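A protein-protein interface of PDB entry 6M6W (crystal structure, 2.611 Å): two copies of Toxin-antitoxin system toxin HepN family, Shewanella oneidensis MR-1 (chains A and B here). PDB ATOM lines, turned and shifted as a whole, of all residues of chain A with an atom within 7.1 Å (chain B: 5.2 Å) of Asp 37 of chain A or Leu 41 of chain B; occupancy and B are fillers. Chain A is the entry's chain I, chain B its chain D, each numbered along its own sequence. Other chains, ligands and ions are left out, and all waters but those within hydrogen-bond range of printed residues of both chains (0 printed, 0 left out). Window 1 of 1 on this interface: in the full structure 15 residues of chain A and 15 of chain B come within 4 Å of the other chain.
The side-chain carboxylate (OD2) of Asp 37 of chain B sits at hydrogen-bond distance from the side-chain hydroxyl (OG) of Ser 38 of chain A (3.0 Å). The side-chain carboxylate of Asp 37 of chain B lies within hydrogen-bond range of the side-chain amide nitrogen of Asn 42 of chain A (3.5 Å). OG of Ser 38 of chain B is in hydrogen-bond range of OD2 of Asp 37 of chain A. The side-chain carboxylate of Asp 37 of chain A is in hydrogen-bond range of the side-chain amide nitrogen of Asn 42 of chain B, 3.2 Å away. The guanidinium group of Arg 45 of chain B is in salt-bridge range of the side-chain carboxylate of Asp 37 of chain A, at 3.2 Å. The backbone carbonyl oxygen (O) of Ala 100 of chain A lies within hydrogen-bond range of the guanidinium group (NE) of Arg 45 of chain B (2.5 Å). OE1 of Gln 105 of chain A is in hydrogen-bond range of NH2 of Arg 45 of chain B (3.4 Å).
The backbone carbonyl oxygen (O) of Ser 38 of chain B is in hydrogen-bond range of the side-chain amide nitrogen (ND2) of Asn 42 of chain B (3.1 Å). NH1 of Arg 45 of chain B is in hydrogen-bond range of OD1 of Asn 42 of chain B (3.0 Å). The backbone carbonyl oxygen (O) of Asn 42 of chain B sits at hydrogen-bond distance from the side-chain sulfur (SG) of Cys 46 of chain B (3.3 Å). OD2 of Asp 32 of chain A sits at hydrogen-bond distance from N of Thr 34 of chain A (2.8 Å). O of Ser 38 of chain A lies within hydrogen-bond range of ND2 of Asn 42 of chain A, at 3.0 Å. O of Arg 97 of chain A lies close to OE1 of Gln 44 of chain A.
Among the printed residues, merely in contact across the chains: Leu 41 of chain A with Asp 37 of chain B (3.5 Å), Ala 100 of chain A with Leu 41 of chain B (3.5 Å), Val 101 of chain A with Arg 45 of chain B (3.6 Å), Gln 44 of chain A with Gln 44 of chain B (3.6 Å), Asp 37 of chain A with Leu 41 of chain B (3.6 Å), Phe 33 of chain A with Ser 38 of chain B (3.8 Å), Thr 34 of chain A with Ser 38 of chain B (3.9 Å) and Leu 41 of chain A with Ile 40 of chain B (3.9 Å).
Of the printed residues of chain B, Phe 33 of chain A touches Ser 38 (3.8 Å). Of chain B, only Ser 38, Leu 41, Asn 42 and Arg 45 come within 4 Å of Asp 37 of chain A. Of the printed residues of chain B, Leu 41 of chain A touches Asp 37 and Ile 40. Of the printed residues of chain B, Ala 100 of chain A touches Leu 41 (3.5 Å) and Arg 45 (2.5 Å). Printed residues of chain B within 4 Å of Gln 105 of chain A: Arg 45 (3.4 Å). Leu 41 of chain B touches two residues of chain A. The nearest residue of chain B that does not touch Asp 37 of chain A is Asp 37 of chain B (4.6 Å). The nearest residue of chain A that does not touch Leu 41 of chain B is Ile 40 of chain A (4.04 Å). The nearest printed residue of chain A that does not touch Gln 44 of chain B is Leu 41 of chain A (4.04 Å).
Of the 11 printed residues of chain B, 7 touch a printed residue of chain A. Of the 21 printed residues of chain A, 10 touch a printed residue of chain B. Hydrophobic or aromatic side chains of chain A that line the printed part of chain B: Phe 33, Leu 41, Ala 100 and Val 101.
Asp 37 of chain A touches Ser 38 of chain B, and with the chains exchanged Ser 38 of chain A touches Asp 37 of chain B. Asp 37 of chain A touches Leu 41 of chain B, and with the chains exchanged Leu 41 of chain A touches Asp 37 of chain B. Asp 37 of chain A touches Asn 42 of chain B, and with the chains exchanged Asn 42 of chain A touches Asp 37 of chain B. Leu 41 of chain A touches Ile 40 of chain B, but with the chains exchanged Ile 40 of chain A does not touch Leu 41 of chain B (4.04 Å). Positions printed for both chains: 36, 37, 38, 39, 40, 41, 42, 43 and 44. Of the 15 pairs that touch across the chains among the printed residues, 7 have their exchanged pair printed and touching as well.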
ATOM      1  N   VAL A  22       0.965  23.103  13.437  1.00  0.00           N
ATOM      2  CA  VAL A  22      -0.434  23.066  13.847  1.00  0.00           C
ATOM      3  C   VAL A  22      -0.615  22.223  15.103  1.00  0.00           C
ATOM      4  O   VAL A  22      -1.416  22.563  15.980  1.00  0.00           O
ATOM      5  CB  VAL A  22      -1.307  22.549  12.688  1.00  0.00           C
ATOM      6  CG1 VAL A  22      -2.622  21.968  13.208  1.00  0.00           C
ATOM      7  CG2 VAL A  22      -1.534  23.642  11.656  1.00  0.00           C
ATOM      8  N   PHE A  29      -4.984  20.632  20.665  1.00  0.00           N
ATOM      9  CA  PHE A  29      -5.208  19.891  19.421  1.00  0.00           C
ATOM     10  C   PHE A  29      -6.445  18.999  19.486  1.00  0.00           C
ATOM     11  O   PHE A  29      -7.282  19.021  18.570  1.00  0.00           O
ATOM     12  CB  PHE A  29      -3.978  19.049  19.069  1.00  0.00           C
ATOM     13  CG  PHE A  29      -4.229  18.015  17.995  1.00  0.00           C
ATOM     14  CD1 PHE A  29      -4.116  18.352  16.657  1.00  0.00           C
ATOM     15  CD2 PHE A  29      -4.551  16.702  18.321  1.00  0.00           C
ATOM     16  CE1 PHE A  29      -4.351  17.413  15.668  1.00  0.00           C
ATOM     17  CE2 PHE A  29      -4.782  15.758  17.330  1.00  0.00           C
ATOM     18  CZ  PHE A  29      -4.680  16.114  16.003  1.00  0.00           C
ATOM     19  N   ASP A  32     -10.006  21.002  19.033  1.00  0.00           N
ATOM     20  CA  ASP A  32     -10.369  21.855  17.904  1.00  0.00           C
ATOM     21  C   ASP A  32     -10.398  20.959  16.674  1.00  0.00           C
ATOM     22  O   ASP A  32      -9.342  20.537  16.189  1.00  0.00           O
ATOM     23  CB  ASP A  32      -9.369  23.002  17.729  1.00  0.00           C
ATOM     24  CG  ASP A  32      -9.697  23.909  16.546  1.00  0.00           C
ATOM     25  OD1 ASP A  32      -9.056  24.974  16.432  1.00  0.00           O
ATOM     26  OD2 ASP A  32     -10.579  23.568  15.731  1.00  0.00           O
ATOM     27  N   PHE A  33     -11.600  20.671  16.163  1.00  0.00           N
ATOM     28  CA  PHE A  33     -11.696  19.779  15.012  1.00  0.00           C
ATOM     29  C   PHE A  33     -10.991  20.348  13.786  1.00  0.00           C
ATOM     30  O   PHE A  33     -10.642  19.585  12.879  1.00  0.00           O
ATOM     31  CB  PHE A  33     -13.167  19.458  14.695  1.00  0.00           C
ATOM     32  CG  PHE A  33     -13.941  20.598  14.072  1.00  0.00           C
ATOM     33  CD1 PHE A  33     -13.902  20.827  12.702  1.00  0.00           C
ATOM     34  CD2 PHE A  33     -14.743  21.414  14.854  1.00  0.00           C
ATOM     35  CE1 PHE A  33     -14.620  21.866  12.132  1.00  0.00           C
ATOM     36  CE2 PHE A  33     -15.468  22.451  14.287  1.00  0.00           C
ATOM     37  CZ  PHE A  33     -15.406  22.676  12.926  1.00  0.00           C
ATOM     38  N   THR A  34     -10.758  21.662  13.746  1.00  0.00           N
ATOM     39  CA  THR A  34     -10.098  22.260  12.590  1.00  0.00           C
ATOM     40  C   THR A  34      -8.609  21.928  12.561  1.00  0.00           C
ATOM     41  O   THR A  34      -8.036  21.714  11.487  1.00  0.00           O
ATOM     42  CB  THR A  34     -10.311  23.776  12.596  1.00  0.00           C
ATOM     43  OG1 THR A  34     -11.597  24.084  12.049  1.00  0.00           O
ATOM     44  CG2 THR A  34      -9.229  24.496  11.795  1.00  0.00           C
ATOM     45  N   LEU A  35      -7.974  21.826  13.729  1.00  0.00           N
ATOM     46  CA  LEU A  35      -6.563  21.460  13.744  1.00  0.00           C
ATOM     47  C   LEU A  35      -6.361  19.967  13.537  1.00  0.00           C
ATOM     48  O   LEU A  35      -5.336  19.556  12.982  1.00  0.00           O
ATOM     49  CB  LEU A  35      -5.916  21.888  15.063  1.00  0.00           C
ATOM     50  CG  LEU A  35      -6.122  23.333  15.513  1.00  0.00           C
ATOM     51  CD1 LEU A  35      -5.803  23.463  16.996  1.00  0.00           C
ATOM     52  CD2 LEU A  35      -5.281  24.289  14.681  1.00  0.00           C
ATOM     53  N   GLN A  36      -7.319  19.147  13.967  1.00  0.00           N
ATOM     54  CA  GLN A  36      -7.292  17.727  13.641  1.00  0.00           C
ATOM     55  C   GLN A  36      -7.440  17.503  12.142  1.00  0.00           C
ATOM     56  O   GLN A  36      -6.719  16.696  11.547  1.00  0.00           O
ATOM     57  CB  GLN A  36      -8.393  17.008  14.419  1.00  0.00           C
ATOM     58  CG  GLN A  36      -8.259  17.175  15.923  1.00  0.00           C
ATOM     59  CD  GLN A  36      -9.533  16.835  16.664  1.00  0.00           C
ATOM     60  OE1 GLN A  36     -10.408  16.147  16.142  1.00  0.00           O
ATOM     61  NE2 GLN A  36      -9.636  17.305  17.902  1.00  0.00           N
ATOM     62  N   ASP A  37      -8.362  18.230  11.507  1.00  0.00           N
ATOM     63  CA  ASP A  37      -8.568  18.083  10.070  1.00  0.00           C
ATOM     64  C   ASP A  37      -7.311  18.465   9.298  1.00  0.00           C
ATOM     65  O   ASP A  37      -6.913  17.776   8.351  1.00  0.00           O
ATOM     66  CB  ASP A  37      -9.761  18.927   9.618  1.00  0.00           C
ATOM     67  CG  ASP A  37     -11.078  18.421  10.180  1.00  0.00           C
ATOM     68  OD1 ASP A  37     -11.104  17.291  10.715  1.00  0.00           O
ATOM     69  OD2 ASP A  37     -12.086  19.156  10.091  1.00  0.00           O
ATOM     70  N   SER A  38      -6.681  19.577   9.683  1.00  0.00           N
ATOM     71  CA  SER A  38      -5.457  20.017   9.018  1.00  0.00           C
ATOM     72  C   SER A  38      -4.357  18.965   9.120  1.00  0.00           C
ATOM     73  O   SER A  38      -3.736  18.599   8.114  1.00  0.00           O
ATOM     74  CB  SER A  38      -4.983  21.341   9.615  1.00  0.00           C
ATOM     75  OG  SER A  38      -3.829  21.814   8.949  1.00  0.00           O
ATOM     76  N   VAL A  39      -4.094  18.477  10.336  1.00  0.00           N
ATOM     77  CA  VAL A  39      -3.062  17.464  10.539  1.00  0.00           C
ATOM     78  C   VAL A  39      -3.375  16.214   9.728  1.00  0.00           C
ATOM     79  O   VAL A  39      -2.499  15.644   9.064  1.00  0.00           O
ATOM     80  CB  VAL A  39      -2.926  17.137  12.039  1.00  0.00           C
ATOM     81  CG1 VAL A  39      -2.171  15.824  12.239  1.00  0.00           C
ATOM     82  CG2 VAL A  39      -2.268  18.286  12.779  1.00  0.00           C
ATOM     83  N   ILE A  40      -4.629  15.760   9.786  1.00  0.00           N
ATOM     84  CA  ILE A  40      -5.007  14.518   9.122  1.00  0.00           C
ATOM     85  C   ILE A  40      -4.851  14.652   7.615  1.00  0.00           C
ATOM     86  O   ILE A  40      -4.346  13.745   6.942  1.00  0.00           O
ATOM     87  CB  ILE A  40      -6.447  14.131   9.504  1.00  0.00           C
ATOM     88  CG1 ILE A  40      -6.527  13.699  10.971  1.00  0.00           C
ATOM     89  CG2 ILE A  40      -6.958  13.027   8.596  1.00  0.00           C
ATOM     90  CD1 ILE A  40      -7.948  13.537  11.476  1.00  0.00           C
ATOM     91  N   LEU A  41      -5.266  15.790   7.062  1.00  0.00           N
ATOM     92  CA  LEU A  41      -5.187  15.968   5.620  1.00  0.00           C
ATOM     93  C   LEU A  41      -3.745  16.163   5.168  1.00  0.00           C
ATOM     94  O   LEU A  41      -3.390  15.774   4.051  1.00  0.00           O
ATOM     95  CB  LEU A  41      -6.070  17.140   5.194  1.00  0.00           C
ATOM     96  CG  LEU A  41      -6.020  17.538   3.716  1.00  0.00           C
ATOM     97  CD1 LEU A  41      -6.638  16.422   2.880  1.00  0.00           C
ATOM     98  CD2 LEU A  41      -6.739  18.847   3.485  1.00  0.00           C
ATOM     99  N   ASN A  42      -2.902  16.754   6.020  1.00  0.00           N
ATOM    100  CA  ASN A  42      -1.488  16.889   5.686  1.00  0.00           C
ATOM    101  C   ASN A  42      -0.752  15.560   5.810  1.00  0.00           C
ATOM    102  O   ASN A  42       0.243  15.339   5.110  1.00  0.00           O
ATOM    103  CB  ASN A  42      -0.822  17.940   6.582  1.00  0.00           C
ATOM    104  CG  ASN A  42      -1.053  19.360   6.097  1.00  0.00           C
ATOM    105  OD1 ASN A  42      -0.851  19.671   4.922  1.00  0.00           O
ATOM    106  ND2 ASN A  42      -1.468  20.234   7.008  1.00  0.00           N
ATOM    107  N   LEU A  43      -1.214  14.666   6.689  1.00  0.00           N
ATOM    108  CA  LEU A  43      -0.644  13.322   6.730  1.00  0.00           C
ATOM    109  C   LEU A  43      -0.951  12.557   5.449  1.00  0.00           C
ATOM    110  O   LEU A  43      -0.080  11.873   4.899  1.00  0.00           O
ATOM    111  CB  LEU A  43      -1.154  12.557   7.953  1.00  0.00           C
ATOM    112  CG  LEU A  43      -0.474  12.894   9.280  1.00  0.00           C
ATOM    113  CD1 LEU A  43      -1.259  12.337  10.459  1.00  0.00           C
ATOM    114  CD2 LEU A  43       0.944  12.343   9.274  1.00  0.00           C
ATOM    115  N   GLN A  44      -2.190  12.659   4.956  1.00  0.00           N
ATOM    116  CA  GLN A  44      -2.542  12.018   3.692  1.00  0.00           C
ATOM    117  C   GLN A  44      -1.702  12.569   2.548  1.00  0.00           C
ATOM    118  O   GLN A  44      -1.180  11.810   1.722  1.00  0.00           O
ATOM    119  CB  GLN A  44      -4.030  12.204   3.390  1.00  0.00           C
ATOM    120  CG  GLN A  44      -4.972  11.586   4.395  1.00  0.00           C
ATOM    121  CD  GLN A  44      -6.404  11.550   3.895  1.00  0.00           C
ATOM    122  OE1 GLN A  44      -7.303  11.070   4.586  1.00  0.00           O
ATOM    123  NE2 GLN A  44      -6.619  12.052   2.679  1.00  0.00           N
ATOM    124  N   ARG A  97      -5.212   6.951   5.191  1.00  0.00           N
ATOM    125  CA  ARG A  97      -6.250   7.413   4.271  1.00  0.00           C
ATOM    126  C   ARG A  97      -7.655   7.108   4.786  1.00  0.00           C
ATOM    127  O   ARG A  97      -8.549   7.959   4.700  1.00  0.00           O
ATOM    128  CB  ARG A  97      -6.041   6.778   2.890  1.00  0.00           C
ATOM    129  CG  ARG A  97      -4.615   6.885   2.371  1.00  0.00           C
ATOM    130  CD  ARG A  97      -4.517   6.712   0.857  1.00  0.00           C
ATOM    131  NE  ARG A  97      -4.668   5.317   0.427  1.00  0.00           N
ATOM    132  CZ  ARG A  97      -4.163   4.829  -0.703  1.00  0.00           C
ATOM    133  NH1 ARG A  97      -3.480   5.621  -1.520  1.00  0.00           N
ATOM    134  NH2 ARG A  97      -4.353   3.559  -1.016  1.00  0.00           N
ATOM    135  N   ILE A  99      -8.661   6.823   7.812  1.00  0.00           N
ATOM    136  CA  ILE A  99      -8.939   7.325   9.152  1.00  0.00           C
ATOM    137  C   ILE A  99      -9.612   8.694   9.125  1.00  0.00           C
ATOM    138  O   ILE A  99     -10.183   9.110  10.146  1.00  0.00           O
ATOM    139  CB  ILE A  99      -7.662   7.371  10.014  1.00  0.00           C
ATOM    140  CG1 ILE A  99      -8.012   7.056  11.468  1.00  0.00           C
ATOM    141  CG2 ILE A  99      -6.989   8.735   9.919  1.00  0.00           C
ATOM    142  CD1 ILE A  99      -8.672   5.703  11.643  1.00  0.00           C
ATOM    143  N   ALA A 100      -9.558   9.406   7.999  1.00  0.00           N
ATOM    144  CA  ALA A 100     -10.386  10.594   7.847  1.00  0.00           C
ATOM    145  C   ALA A 100     -11.859  10.221   7.808  1.00  0.00           C
ATOM    146  O   ALA A 100     -12.704  10.912   8.390  1.00  0.00           O
ATOM    147  CB  ALA A 100      -9.995  11.344   6.577  1.00  0.00           C
ATOM    148  N   VAL A 101     -12.179   9.118   7.141  1.00  0.00           N
ATOM    149  CA  VAL A 101     -13.551   8.723   6.887  1.00  0.00           C
ATOM    150  C   VAL A 101     -13.882   7.425   7.617  1.00  0.00           C
ATOM    151  O   VAL A 101     -14.518   6.527   7.062  1.00  0.00           O
ATOM    152  CB  VAL A 101     -13.795   8.590   5.372  1.00  0.00           C
ATOM    153  CG1 VAL A 101     -13.691   9.947   4.705  1.00  0.00           C
ATOM    154  CG2 VAL A 101     -12.778   7.642   4.754  1.00  0.00           C
ATOM    155  N   GLN A 105     -14.539   8.785  16.063  1.00  0.00           N
ATOM    156  CA  GLN A 105     -13.457   9.594  15.521  1.00  0.00           C
ATOM    157  C   GLN A 105     -12.355   9.780  16.562  1.00  0.00           C
ATOM    158  O   GLN A 105     -11.167   9.799  16.239  1.00  0.00           O
ATOM    159  CB  GLN A 105     -13.993  10.948  15.042  1.00  0.00           C
ATOM    160  CG  GLN A 105     -12.947  12.042  14.867  1.00  0.00           C
ATOM    161  CD  GLN A 105     -12.046  11.822  13.667  1.00  0.00           C
ATOM    162  OE1 GLN A 105     -12.163  12.516  12.657  1.00  0.00           O
ATOM    163  NE2 GLN A 105     -11.133  10.864  13.775  1.00  0.00           N
ATOM    164  N   LEU A 109      -8.080   9.599  17.264  1.00  0.00           N
ATOM    165  CA  LEU A 109      -7.238  10.780  17.396  1.00  0.00           C
ATOM    166  C   LEU A 109      -5.937  10.486  18.131  1.00  0.00           C
ATOM    167  O   LEU A 109      -4.958  11.210  17.933  1.00  0.00           O
ATOM    168  CB  LEU A 109      -8.000  11.914  18.080  1.00  0.00           C
ATOM    169  CG  LEU A 109      -9.133  12.489  17.231  1.00  0.00           C
ATOM    170  CD1 LEU A 109      -9.867  13.575  17.996  1.00  0.00           C
ATOM    171  CD2 LEU A 109      -8.628  13.001  15.887  1.00  0.00           C
ATOM    172  N   GLN B  36      -8.995  25.940   5.226  1.00  0.00           N
ATOM    173  CA  GLN B  36      -9.108  25.305   3.916  1.00  0.00           C
ATOM    174  C   GLN B  36      -8.895  23.802   4.025  1.00  0.00           C
ATOM    175  O   GLN B  36      -9.602  23.020   3.375  1.00  0.00           O
ATOM    176  CB  GLN B  36      -8.140  25.936   2.914  1.00  0.00           C
ATOM    177  CG  GLN B  36      -6.997  26.694   3.527  1.00  0.00           C
ATOM    178  CD  GLN B  36      -6.402  27.727   2.586  1.00  0.00           C
ATOM    179  OE1 GLN B  36      -5.512  27.423   1.791  1.00  0.00           O
ATOM    180  NE2 GLN B  36      -6.889  28.960   2.678  1.00  0.00           N
ATOM    181  N   ASP B  37      -7.929  23.379   4.842  1.00  0.00           N
ATOM    182  CA  ASP B  37      -7.720  21.950   5.050  1.00  0.00           C
ATOM    183  C   ASP B  37      -8.961  21.314   5.655  1.00  0.00           C
ATOM    184  O   ASP B  37      -9.376  20.227   5.238  1.00  0.00           O
ATOM    185  CB  ASP B  37      -6.506  21.706   5.946  1.00  0.00           C
ATOM    186  CG  ASP B  37      -5.202  22.090   5.284  1.00  0.00           C
ATOM    187  OD1 ASP B  37      -5.198  22.325   4.057  1.00  0.00           O
ATOM    188  OD2 ASP B  37      -4.178  22.156   5.996  1.00  0.00           O
ATOM    189  N   SER B  38      -9.552  21.967   6.657  1.00  0.00           N
ATOM    190  CA  SER B  38     -10.777  21.452   7.258  1.00  0.00           C
ATOM    191  C   SER B  38     -11.883  21.331   6.219  1.00  0.00           C
ATOM    192  O   SER B  38     -12.545  20.291   6.119  1.00  0.00           O
ATOM    193  CB  SER B  38     -11.225  22.353   8.408  1.00  0.00           C
ATOM    194  OG  SER B  38     -12.393  21.833   9.023  1.00  0.00           O
ATOM    195  N   VAL B  39     -12.109  22.394   5.448  1.00  0.00           N
ATOM    196  CA  VAL B  39     -13.153  22.366   4.430  1.00  0.00           C
ATOM    197  C   VAL B  39     -12.881  21.261   3.413  1.00  0.00           C
ATOM    198  O   VAL B  39     -13.777  20.479   3.075  1.00  0.00           O
ATOM    199  CB  VAL B  39     -13.278  23.750   3.765  1.00  0.00           C
ATOM    200  CG1 VAL B  39     -13.847  23.635   2.360  1.00  0.00           C
ATOM    201  CG2 VAL B  39     -14.104  24.692   4.639  1.00  0.00           C
ATOM    202  N   ILE B  40     -11.635  21.152   2.941  1.00  0.00           N
ATOM    203  CA  ILE B  40     -11.313  20.175   1.899  1.00  0.00           C
ATOM    204  C   ILE B  40     -11.532  18.754   2.405  1.00  0.00           C
ATOM    205  O   ILE B  40     -12.093  17.906   1.702  1.00  0.00           O
ATOM    206  CB  ILE B  40      -9.864  20.362   1.413  1.00  0.00           C
ATOM    207  CG1 ILE B  40      -9.708  21.631   0.574  1.00  0.00           C
ATOM    208  CG2 ILE B  40      -9.376  19.128   0.652  1.00  0.00           C
ATOM    209  CD1 ILE B  40      -8.263  21.944   0.249  1.00  0.00           C
ATOM    210  N   LEU B  41     -11.111  18.478   3.638  1.00  0.00           N
ATOM    211  CA  LEU B  41     -11.208  17.116   4.144  1.00  0.00           C
ATOM    212  C   LEU B  41     -12.650  16.727   4.455  1.00  0.00           C
ATOM    213  O   LEU B  41     -13.025  15.561   4.282  1.00  0.00           O
ATOM    214  CB  LEU B  41     -10.319  16.960   5.379  1.00  0.00           C
ATOM    215  CG  LEU B  41     -10.450  15.650   6.159  1.00  0.00           C
ATOM    216  CD1 LEU B  41      -9.820  14.571   5.315  1.00  0.00           C
ATOM    217  CD2 LEU B  41      -9.765  15.723   7.510  1.00  0.00           C
ATOM    218  N   ASN B  42     -13.478  17.684   4.885  1.00  0.00           N
ATOM    219  CA  ASN B  42     -14.881  17.383   5.153  1.00  0.00           C
ATOM    220  C   ASN B  42     -15.682  17.218   3.868  1.00  0.00           C
ATOM    221  O   ASN B  42     -16.687  16.500   3.849  1.00  0.00           O
ATOM    222  CB  ASN B  42     -15.489  18.473   6.039  1.00  0.00           C
ATOM    223  CG  ASN B  42     -15.184  18.261   7.514  1.00  0.00           C
ATOM    224  OD1 ASN B  42     -15.382  17.166   8.036  1.00  0.00           O
ATOM    225  ND2 ASN B  42     -14.703  19.303   8.190  1.00  0.00           N
ATOM    226  N   LEU B  43     -15.261  17.885   2.794  1.00  0.00           N
ATOM    227  CA  LEU B  43     -15.831  17.642   1.474  1.00  0.00           C
ATOM    228  C   LEU B  43     -15.483  16.239   0.991  1.00  0.00           C
ATOM    229  O   LEU B  43     -16.329  15.544   0.409  1.00  0.00           O
ATOM    230  CB  LEU B  43     -15.307  18.685   0.490  1.00  0.00           C
ATOM    231  CG  LEU B  43     -15.784  20.140   0.672  1.00  0.00           C
ATOM    232  CD1 LEU B  43     -14.861  21.103  -0.085  1.00  0.00           C
ATOM    233  CD2 LEU B  43     -17.245  20.324   0.265  1.00  0.00           C
ATOM    234  N   GLN B  44     -14.237  15.813   1.236  1.00  0.00           N
ATOM    235  CA  GLN B  44     -13.845  14.429   0.981  1.00  0.00           C
ATOM    236  C   GLN B  44     -14.721  13.456   1.757  1.00  0.00           C
ATOM    237  O   GLN B  44     -15.231  12.479   1.195  1.00  0.00           O
ATOM    238  CB  GLN B  44     -12.384  14.214   1.363  1.00  0.00           C
ATOM    239  CG  GLN B  44     -11.355  14.589   0.319  1.00  0.00           C
ATOM    240  CD  GLN B  44      -9.974  14.043   0.649  1.00  0.00           C
ATOM    241  OE1 GLN B  44      -9.831  13.085   1.409  1.00  0.00           O
ATOM    242  NE2 GLN B  44      -8.951  14.651   0.075  1.00  0.00           N
ATOM    243  N   ARG B  45     -14.870  13.685   3.066  1.00  0.00           N
ATOM    244  CA  ARG B  45     -15.732  12.838   3.884  1.00  0.00           C
ATOM    245  C   ARG B  45     -17.143  12.764   3.314  1.00  0.00           C
ATOM    246  O   ARG B  45     -17.745  11.685   3.258  1.00  0.00           O
ATOM    247  CB  ARG B  45     -15.744  13.341   5.334  1.00  0.00           C
ATOM    248  CG  ARG B  45     -14.419  13.158   6.075  1.00  0.00           C
ATOM    249  CD  ARG B  45     -14.531  13.552   7.544  1.00  0.00           C
ATOM    250  NE  ARG B  45     -13.275  13.351   8.266  1.00  0.00           N
ATOM    251  CZ  ARG B  45     -12.642  14.276   8.979  1.00  0.00           C
ATOM    252  NH1 ARG B  45     -13.124  15.508   9.063  1.00  0.00           N
ATOM    253  NH2 ARG B  45     -11.512  13.965   9.602  1.00  0.00           N
ATOM    254  N   CYS B  46     -17.692  13.906   2.891  1.00  0.00           N
ATOM    255  CA  CYS B  46     -19.003  13.903   2.246  1.00  0.00           C
ATOM    256  C   CYS B  46     -19.005  13.026   0.999  1.00  0.00           C
ATOM    257  O   CYS B  46     -19.922  12.223   0.794  1.00  0.00           O
ATOM    258  CB  CYS B  46     -19.428  15.329   1.892  1.00  0.00           C
ATOM    259  SG  CYS B  46     -19.971  16.345   3.280  1.00  0.00           S
